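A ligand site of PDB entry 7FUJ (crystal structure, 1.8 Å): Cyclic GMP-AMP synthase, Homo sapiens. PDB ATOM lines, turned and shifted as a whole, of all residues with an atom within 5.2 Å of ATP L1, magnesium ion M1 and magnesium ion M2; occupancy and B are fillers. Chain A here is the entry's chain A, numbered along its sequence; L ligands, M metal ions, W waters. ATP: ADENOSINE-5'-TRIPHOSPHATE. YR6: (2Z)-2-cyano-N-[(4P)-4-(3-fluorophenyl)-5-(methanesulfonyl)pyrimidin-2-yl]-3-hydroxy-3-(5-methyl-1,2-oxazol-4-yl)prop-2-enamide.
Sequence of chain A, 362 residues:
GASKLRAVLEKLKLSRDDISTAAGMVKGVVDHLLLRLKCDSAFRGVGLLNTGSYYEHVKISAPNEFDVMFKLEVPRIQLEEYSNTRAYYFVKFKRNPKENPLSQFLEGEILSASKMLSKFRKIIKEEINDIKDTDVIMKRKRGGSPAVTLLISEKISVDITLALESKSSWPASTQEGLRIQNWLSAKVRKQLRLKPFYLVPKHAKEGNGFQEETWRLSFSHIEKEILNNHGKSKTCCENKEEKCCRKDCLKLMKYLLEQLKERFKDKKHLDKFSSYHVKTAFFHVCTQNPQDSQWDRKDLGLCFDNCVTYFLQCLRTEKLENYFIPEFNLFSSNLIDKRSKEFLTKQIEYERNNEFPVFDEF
Residues that only touch magnesium ion M1: Ser 53 (3.8 Å). Of the 20 residues printed, 3 come within 4 Å of magnesium ion M1. The nearest printed residue that does not touch magnesium ion M1 is Gly 52 (4.8 Å).
Magnesium ion M2 is bound by the side-chain carboxylate (OD2) of Asp 159 (2.0 Å), the side-chain carboxylate (OD1) of Asp 67 (2.0 Å), water W7 (2.1 Å), water W2 (2.1 Å), the side-chain carboxylate (OE2) of Glu 65 (2.1 Å) and an oxygen (O2A) of ATP L1 (2.2 Å). Magnesium ion M2 has six donor atoms within binding distance.
Magnesium ion M1 is bound by O2B of ATP L1 (2.0 Å), OD2 of Asp 67 (2.0 Å), OE1 of Glu 65 (2.1 Å), water W1 (2.1 Å), O1G of ATP L1 (2.1 Å) and O2A of ATP L1 (2.2 Å).
The backbone carbonyl oxygen (O) of Ser 53 lies within hydrogen-bond range of the backbone NH (N) of Lys 59, 3.1 Å away. N of Asp 159 is in hydrogen-bond range of O of Phe 66, at 2.9 Å. The side-chain carboxylate of Glu 223 lies within salt-bridge range of the side-chain amino group of Lys 279 (2.7 Å). The side-chain amino group (NZ) of Lys 279 lies within salt-bridge range of the side-chain carboxylate (OE2) of Glu 56 (2.7 Å). The side-chain carboxylate (OE2) of Glu 223 is in hydrogen-bond range of the side-chain hydroxyl (OH) of Tyr 276 (2.7 Å).
An oxygen (O3') of ATP L1 sits at hydrogen-bond distance from the side-chain amino group (NZ) of Lys 279 (2.9 Å). NZ of Lys 254 lies within salt-bridge range of O3G of ATP L1. An oxygen (O2') of ATP L1 sits at hydrogen-bond distance from the side-chain hydroxyl (OG) of Ser 220 (2.7 Å). N of Ser 53 sits close to O2B of ATP L1, 3.0 Å away. OE1 of Glu 223 sits at hydrogen-bond distance from O2' of ATP L1 (2.6 Å). The guanidinium group (NH1) of Arg 216 is in hydrogen-bond range of an oxygen (O5) of YR6 L2, at 2.7 Å. NH1 of Arg 216 sits close to N3 of ATP L1. O2G of ATP L1 lies within hydrogen-bond range of OG of Ser 275, 2.7 Å away. OG of Ser 53 lies within hydrogen-bond range of O3G of ATP L1, at 2.7 Å.
An oxygen (O25) of YR6 L2 lies close to an oxygen (O4') of ATP L1 (3.4 Å).
Water W1 lies within hydrogen-bond range of the side-chain hydroxyl of Ser 53 and the backbone carbonyl oxygen of Glu 65. Water W3 bridges N7 of ATP L1 (2.7 Å) and O13 of YR6 L2 (3.2 Å). Water W11 lies within hydrogen-bond range of an oxygen (O1A) of ATP L1 (2.7 Å), the side-chain hydroxyl (OG) of Ser 275 (2.9 Å) and the backbone NH (N) of Tyr 276 (3.3 Å). Water W8 lies within hydrogen-bond range of the side-chain carboxylate (OE1) of Glu 56 (2.7 Å) and an oxygen (O1B) of ATP L1 (2.8 Å). Water W4 lies within hydrogen-bond range of an oxygen (O3G) of ATP L1 (2.9 Å), the side-chain carboxylate (OE2) of Glu 258 (3.0 Å) and the side-chain amino group (NZ) of Lys 59 (3.0 Å). Water W6 lies within hydrogen-bond range of the side-chain carboxylate of Glu 258 (2.7 Å), the side-chain amino group of Lys 254 (2.8 Å) and an oxygen (O2G) of ATP L1 (3.1 Å).
Three residues have an atom within 4 Å of magnesium ion M2: Glu 65, Asp 67 and Asp 159. The nearest printed residue that does not touch magnesium ion M2 is Phe 66 (4.9 Å).
Residues that only touch ATP L1: Tyr 276 (3.4 Å), Gly 52 (3.5 Å) and Lys 59 (3.999 Å). Hydrophobic or aromatic side chains that line ATP L1: Tyr 276. Of the 20 residues printed, 12 come within 4 Å of ATP L1. The nearest printed residue that does not touch ATP L1 is Asp 159 (4.2 Å).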
ATOM      1  N   GLY A  52      13.749 -20.459 -24.343  1.00  0.00           N
ATOM      2  CA  GLY A  52      14.055 -21.266 -23.142  1.00  0.00           C
ATOM      3  C   GLY A  52      15.487 -21.105 -22.686  1.00  0.00           C
ATOM      4  O   GLY A  52      16.210 -20.174 -23.129  1.00  0.00           O
ATOM      5  N   SER A  53      15.890 -21.995 -21.790  1.00  0.00           N
ATOM      6  CA  SER A  53      16.999 -21.767 -20.850  1.00  0.00           C
ATOM      7  C   SER A  53      18.335 -21.763 -21.595  1.00  0.00           C
ATOM      8  O   SER A  53      19.225 -21.014 -21.188  1.00  0.00           O
ATOM      9  CB  SER A  53      16.930 -22.812 -19.746  1.00  0.00           C
ATOM     10  OG  SER A  53      17.137 -24.130 -20.240  1.00  0.00           O
ATOM     11  N   TYR A  54      18.484 -22.537 -22.646  1.00  0.00           N
ATOM     12  CA  TYR A  54      19.795 -22.562 -23.335  1.00  0.00           C
ATOM     13  C   TYR A  54      20.067 -21.175 -23.942  1.00  0.00           C
ATOM     14  O   TYR A  54      21.149 -20.647 -23.691  1.00  0.00           O
ATOM     15  CB  TYR A  54      19.836 -23.576 -24.455  1.00  0.00           C
ATOM     16  CG  TYR A  54      21.181 -23.602 -25.114  1.00  0.00           C
ATOM     17  CD1 TYR A  54      22.220 -24.324 -24.577  1.00  0.00           C
ATOM     18  CD2 TYR A  54      21.425 -22.849 -26.243  1.00  0.00           C
ATOM     19  CE1 TYR A  54      23.456 -24.350 -25.173  1.00  0.00           C
ATOM     20  CE2 TYR A  54      22.672 -22.844 -26.854  1.00  0.00           C
ATOM     21  CZ  TYR A  54      23.687 -23.618 -26.323  1.00  0.00           C
ATOM     22  OH  TYR A  54      24.892 -23.652 -26.972  1.00  0.00           O
ATOM     23  N   GLU A  56      18.631 -18.364 -23.121  1.00  0.00           N
ATOM     24  CA  GLU A  56      18.635 -17.393 -21.996  1.00  0.00           C
ATOM     25  C   GLU A  56      19.911 -17.499 -21.155  1.00  0.00           C
ATOM     26  O   GLU A  56      20.080 -16.672 -20.232  1.00  0.00           O
ATOM     27  CB  GLU A  56      17.404 -17.601 -21.110  1.00  0.00           C
ATOM     28  CG  GLU A  56      16.110 -17.229 -21.798  1.00  0.00           C
ATOM     29  CD  GLU A  56      14.863 -17.798 -21.147  1.00  0.00           C
ATOM     30  OE1 GLU A  56      14.996 -18.723 -20.299  1.00  0.00           O
ATOM     31  OE2 GLU A  56      13.762 -17.356 -21.499  1.00  0.00           O
ATOM     32  N   LYS A  59      20.446 -22.416 -18.710  1.00  0.00           N
ATOM     33  CA  LYS A  59      20.548 -23.908 -18.712  1.00  0.00           C
ATOM     34  C   LYS A  59      21.626 -24.325 -17.715  1.00  0.00           C
ATOM     35  O   LYS A  59      22.682 -23.661 -17.656  1.00  0.00           O
ATOM     36  CB  LYS A  59      20.856 -24.495 -20.101  1.00  0.00           C
ATOM     37  CG  LYS A  59      20.847 -26.014 -20.193  1.00  0.00           C
ATOM     38  CD  LYS A  59      19.470 -26.568 -20.379  1.00  0.00           C
ATOM     39  CE  LYS A  59      19.419 -28.077 -20.339  1.00  0.00           C
ATOM     40  NZ  LYS A  59      19.857 -28.580 -19.009  1.00  0.00           N
ATOM     41  N   GLU A  65      19.041 -30.011 -23.565  1.00  0.00           N
ATOM     42  CA  GLU A  65      17.604 -29.694 -23.804  1.00  0.00           C
ATOM     43  C   GLU A  65      17.501 -28.278 -24.350  1.00  0.00           C
ATOM     44  O   GLU A  65      17.894 -27.328 -23.627  1.00  0.00           O
ATOM     45  CB  GLU A  65      16.764 -29.868 -22.525  1.00  0.00           C
ATOM     46  CG  GLU A  65      15.262 -30.050 -22.817  1.00  0.00           C
ATOM     47  CD  GLU A  65      14.383 -28.809 -22.789  1.00  0.00           C
ATOM     48  OE1 GLU A  65      14.877 -27.770 -22.382  1.00  0.00           O
ATOM     49  OE2 GLU A  65      13.227 -28.871 -23.267  1.00  0.00           O
ATOM     50  N   PHE A  66      17.059 -28.186 -25.596  1.00  0.00           N
ATOM     51  CA  PHE A  66      16.922 -26.952 -26.413  1.00  0.00           C
ATOM     52  C   PHE A  66      15.443 -26.747 -26.722  1.00  0.00           C
ATOM     53  O   PHE A  66      14.726 -27.740 -26.926  1.00  0.00           O
ATOM     54  CB  PHE A  66      17.728 -27.076 -27.708  1.00  0.00           C
ATOM     55  CG  PHE A  66      19.222 -27.151 -27.515  1.00  0.00           C
ATOM     56  CD1 PHE A  66      19.816 -28.314 -27.011  1.00  0.00           C
ATOM     57  CD2 PHE A  66      20.038 -26.073 -27.818  1.00  0.00           C
ATOM     58  CE1 PHE A  66      21.184 -28.377 -26.810  1.00  0.00           C
ATOM     59  CE2 PHE A  66      21.415 -26.143 -27.653  1.00  0.00           C
ATOM     60  CZ  PHE A  66      21.984 -27.285 -27.145  1.00  0.00           C
ATOM     61  N   ASP A  67      15.011 -25.498 -26.755  1.00  0.00           N
ATOM     62  CA  ASP A  67      13.628 -25.098 -27.078  1.00  0.00           C
ATOM     63  C   ASP A  67      13.654 -24.178 -28.307  1.00  0.00           C
ATOM     64  O   ASP A  67      14.472 -23.229 -28.365  1.00  0.00           O
ATOM     65  CB  ASP A  67      12.945 -24.485 -25.856  1.00  0.00           C
ATOM     66  CG  ASP A  67      12.998 -25.423 -24.669  1.00  0.00           C
ATOM     67  OD1 ASP A  67      12.224 -26.453 -24.687  1.00  0.00           O
ATOM     68  OD2 ASP A  67      13.830 -25.176 -23.756  1.00  0.00           O
ATOM     69  N   ASP A 159      12.766 -29.528 -28.048  1.00  0.00           N
ATOM     70  CA  ASP A 159      11.310 -29.258 -28.033  1.00  0.00           C
ATOM     71  C   ASP A 159      11.041 -28.245 -29.121  1.00  0.00           C
ATOM     72  O   ASP A 159      11.633 -27.157 -29.072  1.00  0.00           O
ATOM     73  CB  ASP A 159      10.785 -28.719 -26.689  1.00  0.00           C
ATOM     74  CG  ASP A 159      10.853 -29.732 -25.554  1.00  0.00           C
ATOM     75  OD1 ASP A 159      10.866 -30.962 -25.883  1.00  0.00           O
ATOM     76  OD2 ASP A 159      10.928 -29.301 -24.361  1.00  0.00           O
ATOM     77  N   ARG A 216      -2.990 -21.555 -26.429  1.00  0.00           N
ATOM     78  CA  ARG A 216      -2.610 -20.849 -25.166  1.00  0.00           C
ATOM     79  C   ARG A 216      -1.609 -19.744 -25.494  1.00  0.00           C
ATOM     80  O   ARG A 216      -0.742 -19.956 -26.355  1.00  0.00           O
ATOM     81  CB  ARG A 216      -2.049 -21.812 -24.126  1.00  0.00           C
ATOM     82  CG  ARG A 216      -2.014 -21.213 -22.726  1.00  0.00           C
ATOM     83  CD  ARG A 216      -0.903 -21.813 -21.859  1.00  0.00           C
ATOM     84  NE  ARG A 216       0.346 -21.302 -22.379  1.00  0.00           N
ATOM     85  CZ  ARG A 216       1.475 -21.982 -22.549  1.00  0.00           C
ATOM     86  NH1 ARG A 216       2.503 -21.377 -23.123  1.00  0.00           N
ATOM     87  NH2 ARG A 216       1.594 -23.244 -22.196  1.00  0.00           N
ATOM     88  N   LEU A 217      -1.720 -18.612 -24.814  1.00  0.00           N
ATOM     89  CA  LEU A 217      -0.763 -17.500 -25.056  1.00  0.00           C
ATOM     90  C   LEU A 217       0.667 -17.977 -24.719  1.00  0.00           C
ATOM     91  O   LEU A 217       0.827 -18.811 -23.763  1.00  0.00           O
ATOM     92  CB  LEU A 217      -1.141 -16.291 -24.208  1.00  0.00           C
ATOM     93  CG  LEU A 217      -2.449 -15.601 -24.542  1.00  0.00           C
ATOM     94  CD1 LEU A 217      -2.699 -14.440 -23.612  1.00  0.00           C
ATOM     95  CD2 LEU A 217      -2.450 -15.134 -25.971  1.00  0.00           C
ATOM     96  N   SER A 220       7.365 -16.438 -24.526  1.00  0.00           N
ATOM     97  CA  SER A 220       8.751 -16.970 -24.472  1.00  0.00           C
ATOM     98  C   SER A 220       9.750 -15.965 -25.066  1.00  0.00           C
ATOM     99  O   SER A 220      10.857 -15.875 -24.552  1.00  0.00           O
ATOM    100  CB  SER A 220       8.843 -18.283 -25.155  1.00  0.00           C
ATOM    101  OG  SER A 220       7.968 -19.182 -24.538  1.00  0.00           O
ATOM    102  N   GLU A 223      10.252 -13.211 -22.407  1.00  0.00           N
ATOM    103  CA  GLU A 223      11.046 -13.791 -21.297  1.00  0.00           C
ATOM    104  C   GLU A 223      12.524 -13.834 -21.691  1.00  0.00           C
ATOM    105  O   GLU A 223      13.374 -13.468 -20.858  1.00  0.00           O
ATOM    106  CB  GLU A 223      10.551 -15.196 -20.958  1.00  0.00           C
ATOM    107  CG  GLU A 223       9.124 -15.203 -20.515  1.00  0.00           C
ATOM    108  CD  GLU A 223       8.504 -16.584 -20.402  1.00  0.00           C
ATOM    109  OE1 GLU A 223       9.273 -17.587 -20.464  1.00  0.00           O
ATOM    110  OE2 GLU A 223       7.250 -16.647 -20.227  1.00  0.00           O
ATOM    111  N   LYS A 254      16.580 -23.251 -10.099  1.00  0.00           N
ATOM    112  CA  LYS A 254      16.360 -24.353 -11.060  1.00  0.00           C
ATOM    113  C   LYS A 254      16.973 -25.646 -10.513  1.00  0.00           C
ATOM    114  O   LYS A 254      16.328 -26.698 -10.606  1.00  0.00           O
ATOM    115  CB  LYS A 254      16.955 -23.994 -12.421  1.00  0.00           C
ATOM    116  CG  LYS A 254      16.171 -22.912 -13.167  1.00  0.00           C
ATOM    117  CD  LYS A 254      16.829 -22.379 -14.406  1.00  0.00           C
ATOM    118  CE  LYS A 254      17.032 -23.417 -15.513  1.00  0.00           C
ATOM    119  NZ  LYS A 254      15.762 -24.010 -15.966  1.00  0.00           N
ATOM    120  N   GLU A 258      15.279 -29.198  -9.713  1.00  0.00           N
ATOM    121  CA  GLU A 258      15.752 -30.391 -10.485  1.00  0.00           C
ATOM    122  C   GLU A 258      16.181 -31.490  -9.489  1.00  0.00           C
ATOM    123  O   GLU A 258      15.799 -32.657  -9.690  1.00  0.00           O
ATOM    124  CB  GLU A 258      16.872 -30.040 -11.479  1.00  0.00           C
ATOM    125  CG  GLU A 258      16.366 -29.451 -12.805  1.00  0.00           C
ATOM    126  CD  GLU A 258      17.463 -29.224 -13.852  1.00  0.00           C
ATOM    127  OE1 GLU A 258      18.470 -29.996 -13.822  1.00  0.00           O
ATOM    128  OE2 GLU A 258      17.328 -28.289 -14.714  1.00  0.00           O
ATOM    129  N   SER A 275      10.202 -26.193 -14.064  1.00  0.00           N
ATOM    130  CA  SER A 275      11.187 -25.084 -14.043  1.00  0.00           C
ATOM    131  C   SER A 275      10.450 -23.775 -14.309  1.00  0.00           C
ATOM    132  O   SER A 275      10.923 -22.761 -13.815  1.00  0.00           O
ATOM    133  CB  SER A 275      12.326 -25.321 -15.033  1.00  0.00           C
ATOM    134  OG  SER A 275      11.866 -25.241 -16.380  1.00  0.00           O
ATOM    135  N   TYR A 276       9.328 -23.769 -15.018  1.00  0.00           N
ATOM    136  CA  TYR A 276       8.576 -22.530 -15.335  1.00  0.00           C
ATOM    137  C   TYR A 276       8.001 -21.929 -14.045  1.00  0.00           C
ATOM    138  O   TYR A 276       7.839 -20.716 -13.996  1.00  0.00           O
ATOM    139  CB  TYR A 276       7.457 -22.741 -16.356  1.00  0.00           C
ATOM    140  CG  TYR A 276       6.951 -21.449 -16.929  1.00  0.00           C
ATOM    141  CD1 TYR A 276       7.798 -20.581 -17.617  1.00  0.00           C
ATOM    142  CD2 TYR A 276       5.655 -21.023 -16.705  1.00  0.00           C
ATOM    143  CE1 TYR A 276       7.343 -19.375 -18.117  1.00  0.00           C
ATOM    144  CE2 TYR A 276       5.192 -19.822 -17.201  1.00  0.00           C
ATOM    145  CZ  TYR A 276       6.027 -19.010 -17.922  1.00  0.00           C
ATOM    146  OH  TYR A 276       5.569 -17.806 -18.387  1.00  0.00           O
ATOM    147  N   LYS A 279      10.954 -20.080 -12.690  1.00  0.00           N
ATOM    148  CA  LYS A 279      11.275 -18.939 -13.610  1.00  0.00           C
ATOM    149  C   LYS A 279      10.286 -17.804 -13.338  1.00  0.00           C
ATOM    150  O   LYS A 279      10.716 -16.619 -13.211  1.00  0.00           O
ATOM    151  CB  LYS A 279      11.200 -19.361 -15.081  1.00  0.00           C
ATOM    152  CG  LYS A 279      11.766 -18.334 -16.054  1.00  0.00           C
ATOM    153  CD  LYS A 279      11.378 -18.687 -17.494  1.00  0.00           C
ATOM    154  CE  LYS A 279      12.120 -17.891 -18.533  1.00  0.00           C
ATOM    155  NZ  LYS A 279      11.794 -18.275 -19.912  1.00  0.00           N
ATOM    156  N   ASN A 322       0.985 -16.076 -13.413  1.00  0.00           N
ATOM    157  CA  ASN A 322       1.691 -15.919 -14.704  1.00  0.00           C
ATOM    158  C   ASN A 322       2.167 -14.464 -14.775  1.00  0.00           C
ATOM    159  O   ASN A 322       1.382 -13.542 -14.427  1.00  0.00           O
ATOM    160  CB  ASN A 322       0.835 -16.376 -15.861  1.00  0.00           C
ATOM    161  CG  ASN A 322       1.493 -16.191 -17.196  1.00  0.00           C
ATOM    162  OD1 ASN A 322       1.786 -15.064 -17.617  1.00  0.00           O
ATOM    163  ND2 ASN A 322       1.698 -17.297 -17.894  1.00  0.00           N
ATOM    164  N   LEU A 330      -0.814 -20.266 -11.632  1.00  0.00           N
ATOM    165  CA  LEU A 330      -0.076 -21.519 -11.945  1.00  0.00           C
ATOM    166  C   LEU A 330      -0.212 -22.523 -10.799  1.00  0.00           C
ATOM    167  O   LEU A 330      -0.009 -23.711 -11.069  1.00  0.00           O
ATOM    168  CB  LEU A 330       1.400 -21.239 -12.210  1.00  0.00           C
ATOM    169  CG  LEU A 330       1.705 -20.314 -13.386  1.00  0.00           C
ATOM    170  CD1 LEU A 330       3.179 -19.949 -13.426  1.00  0.00           C
ATOM    171  CD2 LEU A 330       1.313 -20.957 -14.687  1.00  0.00           C
HETATM  172  PG  ATP L   1      14.751 -25.926 -18.562  1.00  0.00           P
HETATM  173  O1G ATP L   1      14.493 -26.540 -19.922  1.00  0.00           O
HETATM  174  O2G ATP L   1      13.990 -26.589 -17.441  1.00  0.00           O
HETATM  175  O3G ATP L   1      16.195 -25.674 -18.266  1.00  0.00           O
HETATM  176  PB  ATP L   1      13.159 -23.812 -19.809  1.00  0.00           P
HETATM  177  O1B ATP L   1      12.748 -22.415 -19.520  1.00  0.00           O
HETATM  178  O2B ATP L   1      13.920 -24.086 -21.093  1.00  0.00           O
HETATM  179  O3B ATP L   1      14.090 -24.409 -18.654  1.00  0.00           O
HETATM  180  PA  ATP L   1      11.046 -25.677 -20.744  1.00  0.00           P
HETATM  181  O1A ATP L   1      10.168 -26.589 -19.960  1.00  0.00           O
HETATM  182  O2A ATP L   1      12.042 -26.249 -21.723  1.00  0.00           O
HETATM  183  O3A ATP L   1      11.926 -24.821 -19.713  1.00  0.00           O
HETATM  184  O5' ATP L   1      10.142 -24.590 -21.436  1.00  0.00           O
HETATM  185  C5' ATP L   1      10.641 -23.789 -22.548  1.00  0.00           C
HETATM  186  C4' ATP L   1       9.965 -22.449 -22.508  1.00  0.00           C
HETATM  187  O4' ATP L   1       8.550 -22.621 -22.763  1.00  0.00           O
HETATM  188  C3' ATP L   1      10.017 -21.695 -21.177  1.00  0.00           C
HETATM  189  O3' ATP L   1      11.176 -20.913 -20.928  1.00  0.00           O
HETATM  190  C2' ATP L   1       8.774 -20.793 -21.288  1.00  0.00           C
HETATM  191  O2' ATP L   1       9.008 -19.636 -22.035  1.00  0.00           O
HETATM  192  C1' ATP L   1       7.779 -21.710 -21.995  1.00  0.00           C
HETATM  193  N9  ATP L   1       6.922 -22.438 -21.061  1.00  0.00           N
HETATM  194  C8  ATP L   1       7.145 -23.653 -20.427  1.00  0.00           C
HETATM  195  N7  ATP L   1       6.188 -23.981 -19.596  1.00  0.00           N
HETATM  196  C5  ATP L   1       5.254 -22.945 -19.708  1.00  0.00           C
HETATM  197  C6  ATP L   1       3.996 -22.730 -19.103  1.00  0.00           C
HETATM  198  N6  ATP L   1       3.432 -23.565 -18.225  1.00  0.00           N
HETATM  199  N1  ATP L   1       3.329 -21.615 -19.455  1.00  0.00           N
HETATM  200  C2  ATP L   1       3.889 -20.783 -20.341  1.00  0.00           C
HETATM  201  N3  ATP L   1       5.072 -20.868 -20.952  1.00  0.00           N
HETATM  202  C4  ATP L   1       5.696 -21.999 -20.598  1.00  0.00           C
HETATM  203  C10 YR6 L   2       3.757 -27.431 -19.920  1.00  0.00           C
HETATM  204  O14 YR6 L   2       1.671 -27.589 -18.357  1.00  0.00           O
HETATM  205  C15 YR6 L   2       5.014 -27.802 -20.475  1.00  0.00           C
HETATM  206  C16 YR6 L   2       5.847 -28.950 -20.052  1.00  0.00           C
HETATM  207  C17 YR6 L   2       5.369 -30.263 -20.151  1.00  0.00           C
HETATM  208  C18 YR6 L   2       6.154 -31.335 -19.764  1.00  0.00           C
HETATM  209  C19 YR6 L   2       7.456 -31.141 -19.327  1.00  0.00           C
HETATM  210  C20 YR6 L   2       7.930 -29.842 -19.290  1.00  0.00           C
HETATM  211  C21 YR6 L   2       7.163 -28.746 -19.624  1.00  0.00           C
HETATM  212  C24 YR6 L   2       7.206 -24.250 -24.941  1.00  0.00           C
HETATM  213  C26 YR6 L   2       8.148 -23.681 -25.864  1.00  0.00           C
HETATM  214  C27 YR6 L   2       9.035 -24.288 -26.713  1.00  0.00           C
HETATM  215  N1  YR6 L   2       5.364 -21.348 -25.438  1.00  0.00           N
HETATM  216  C2  YR6 L   2       5.685 -22.367 -25.037  1.00  0.00           C
HETATM  217  C3  YR6 L   2       6.045 -23.637 -24.517  1.00  0.00           C
HETATM  218  C4  YR6 L   2       5.151 -24.148 -23.486  1.00  0.00           C
HETATM  219  O5  YR6 L   2       4.131 -23.515 -23.179  1.00  0.00           O
HETATM  220  N6  YR6 L   2       5.436 -25.371 -22.992  1.00  0.00           N
HETATM  221  C7  YR6 L   2       4.813 -26.076 -21.990  1.00  0.00           C
HETATM  222  N8  YR6 L   2       3.655 -25.616 -21.508  1.00  0.00           N
HETATM  223  C9  YR6 L   2       3.133 -26.326 -20.506  1.00  0.00           C
HETATM  224  S11 YR6 L   2       2.952 -28.217 -18.534  1.00  0.00           S
HETATM  225  C12 YR6 L   2       2.696 -29.890 -18.943  1.00  0.00           C
HETATM  226  O13 YR6 L   2       3.880 -28.156 -17.435  1.00  0.00           O
HETATM  227  F22 YR6 L   2       9.203 -29.631 -18.879  1.00  0.00           F
HETATM  228  N23 YR6 L   2       5.537 -27.104 -21.509  1.00  0.00           N
HETATM  229  O25 YR6 L   2       7.584 -25.411 -24.452  1.00  0.00           O
HETATM  230  O28 YR6 L   2       9.797 -23.355 -27.301  1.00  0.00           O
HETATM  231  N29 YR6 L   2       9.424 -22.087 -26.817  1.00  0.00           N
HETATM  232  C30 YR6 L   2       8.486 -22.318 -25.945  1.00  0.00           C
HETATM  233  C31 YR6 L   2       9.288 -25.683 -27.112  1.00  0.00           C
HETATM  234 MG    MG M   1      14.188 -25.895 -21.897  1.00  0.00          MG
HETATM  235 MG    MG M   2      11.498 -27.702 -23.248  1.00  0.00          MG
HETATM  236  O   HOH W   1      16.183 -25.463 -22.301  1.00  0.00           O
HETATM  237  O   HOH W   2       9.542 -26.983 -23.293  1.00  0.00           O
HETATM  238  O   HOH W   3       6.176 -25.977 -17.783  1.00  0.00           O
HETATM  239  O   HOH W   4      18.510 -26.769 -17.009  1.00  0.00           O
HETATM  240  O   HOH W   5      11.467 -22.619 -16.963  1.00  0.00           O
HETATM  241  O   HOH W   6      15.396 -26.414 -14.652  1.00  0.00           O
HETATM  242  O   HOH W   7      10.896 -28.892 -21.669  1.00  0.00           O
HETATM  243  O   HOH W   8      14.543 -20.555 -18.391  1.00  0.00           O
HETATM  244  O   HOH W   9       1.315 -20.156 -18.101  1.00  0.00           O
HETATM  245  O   HOH W  10      12.024 -28.365 -18.048  1.00  0.00           O
HETATM  246  O   HOH W  11       9.216 -25.903 -17.491  1.00  0.00           O
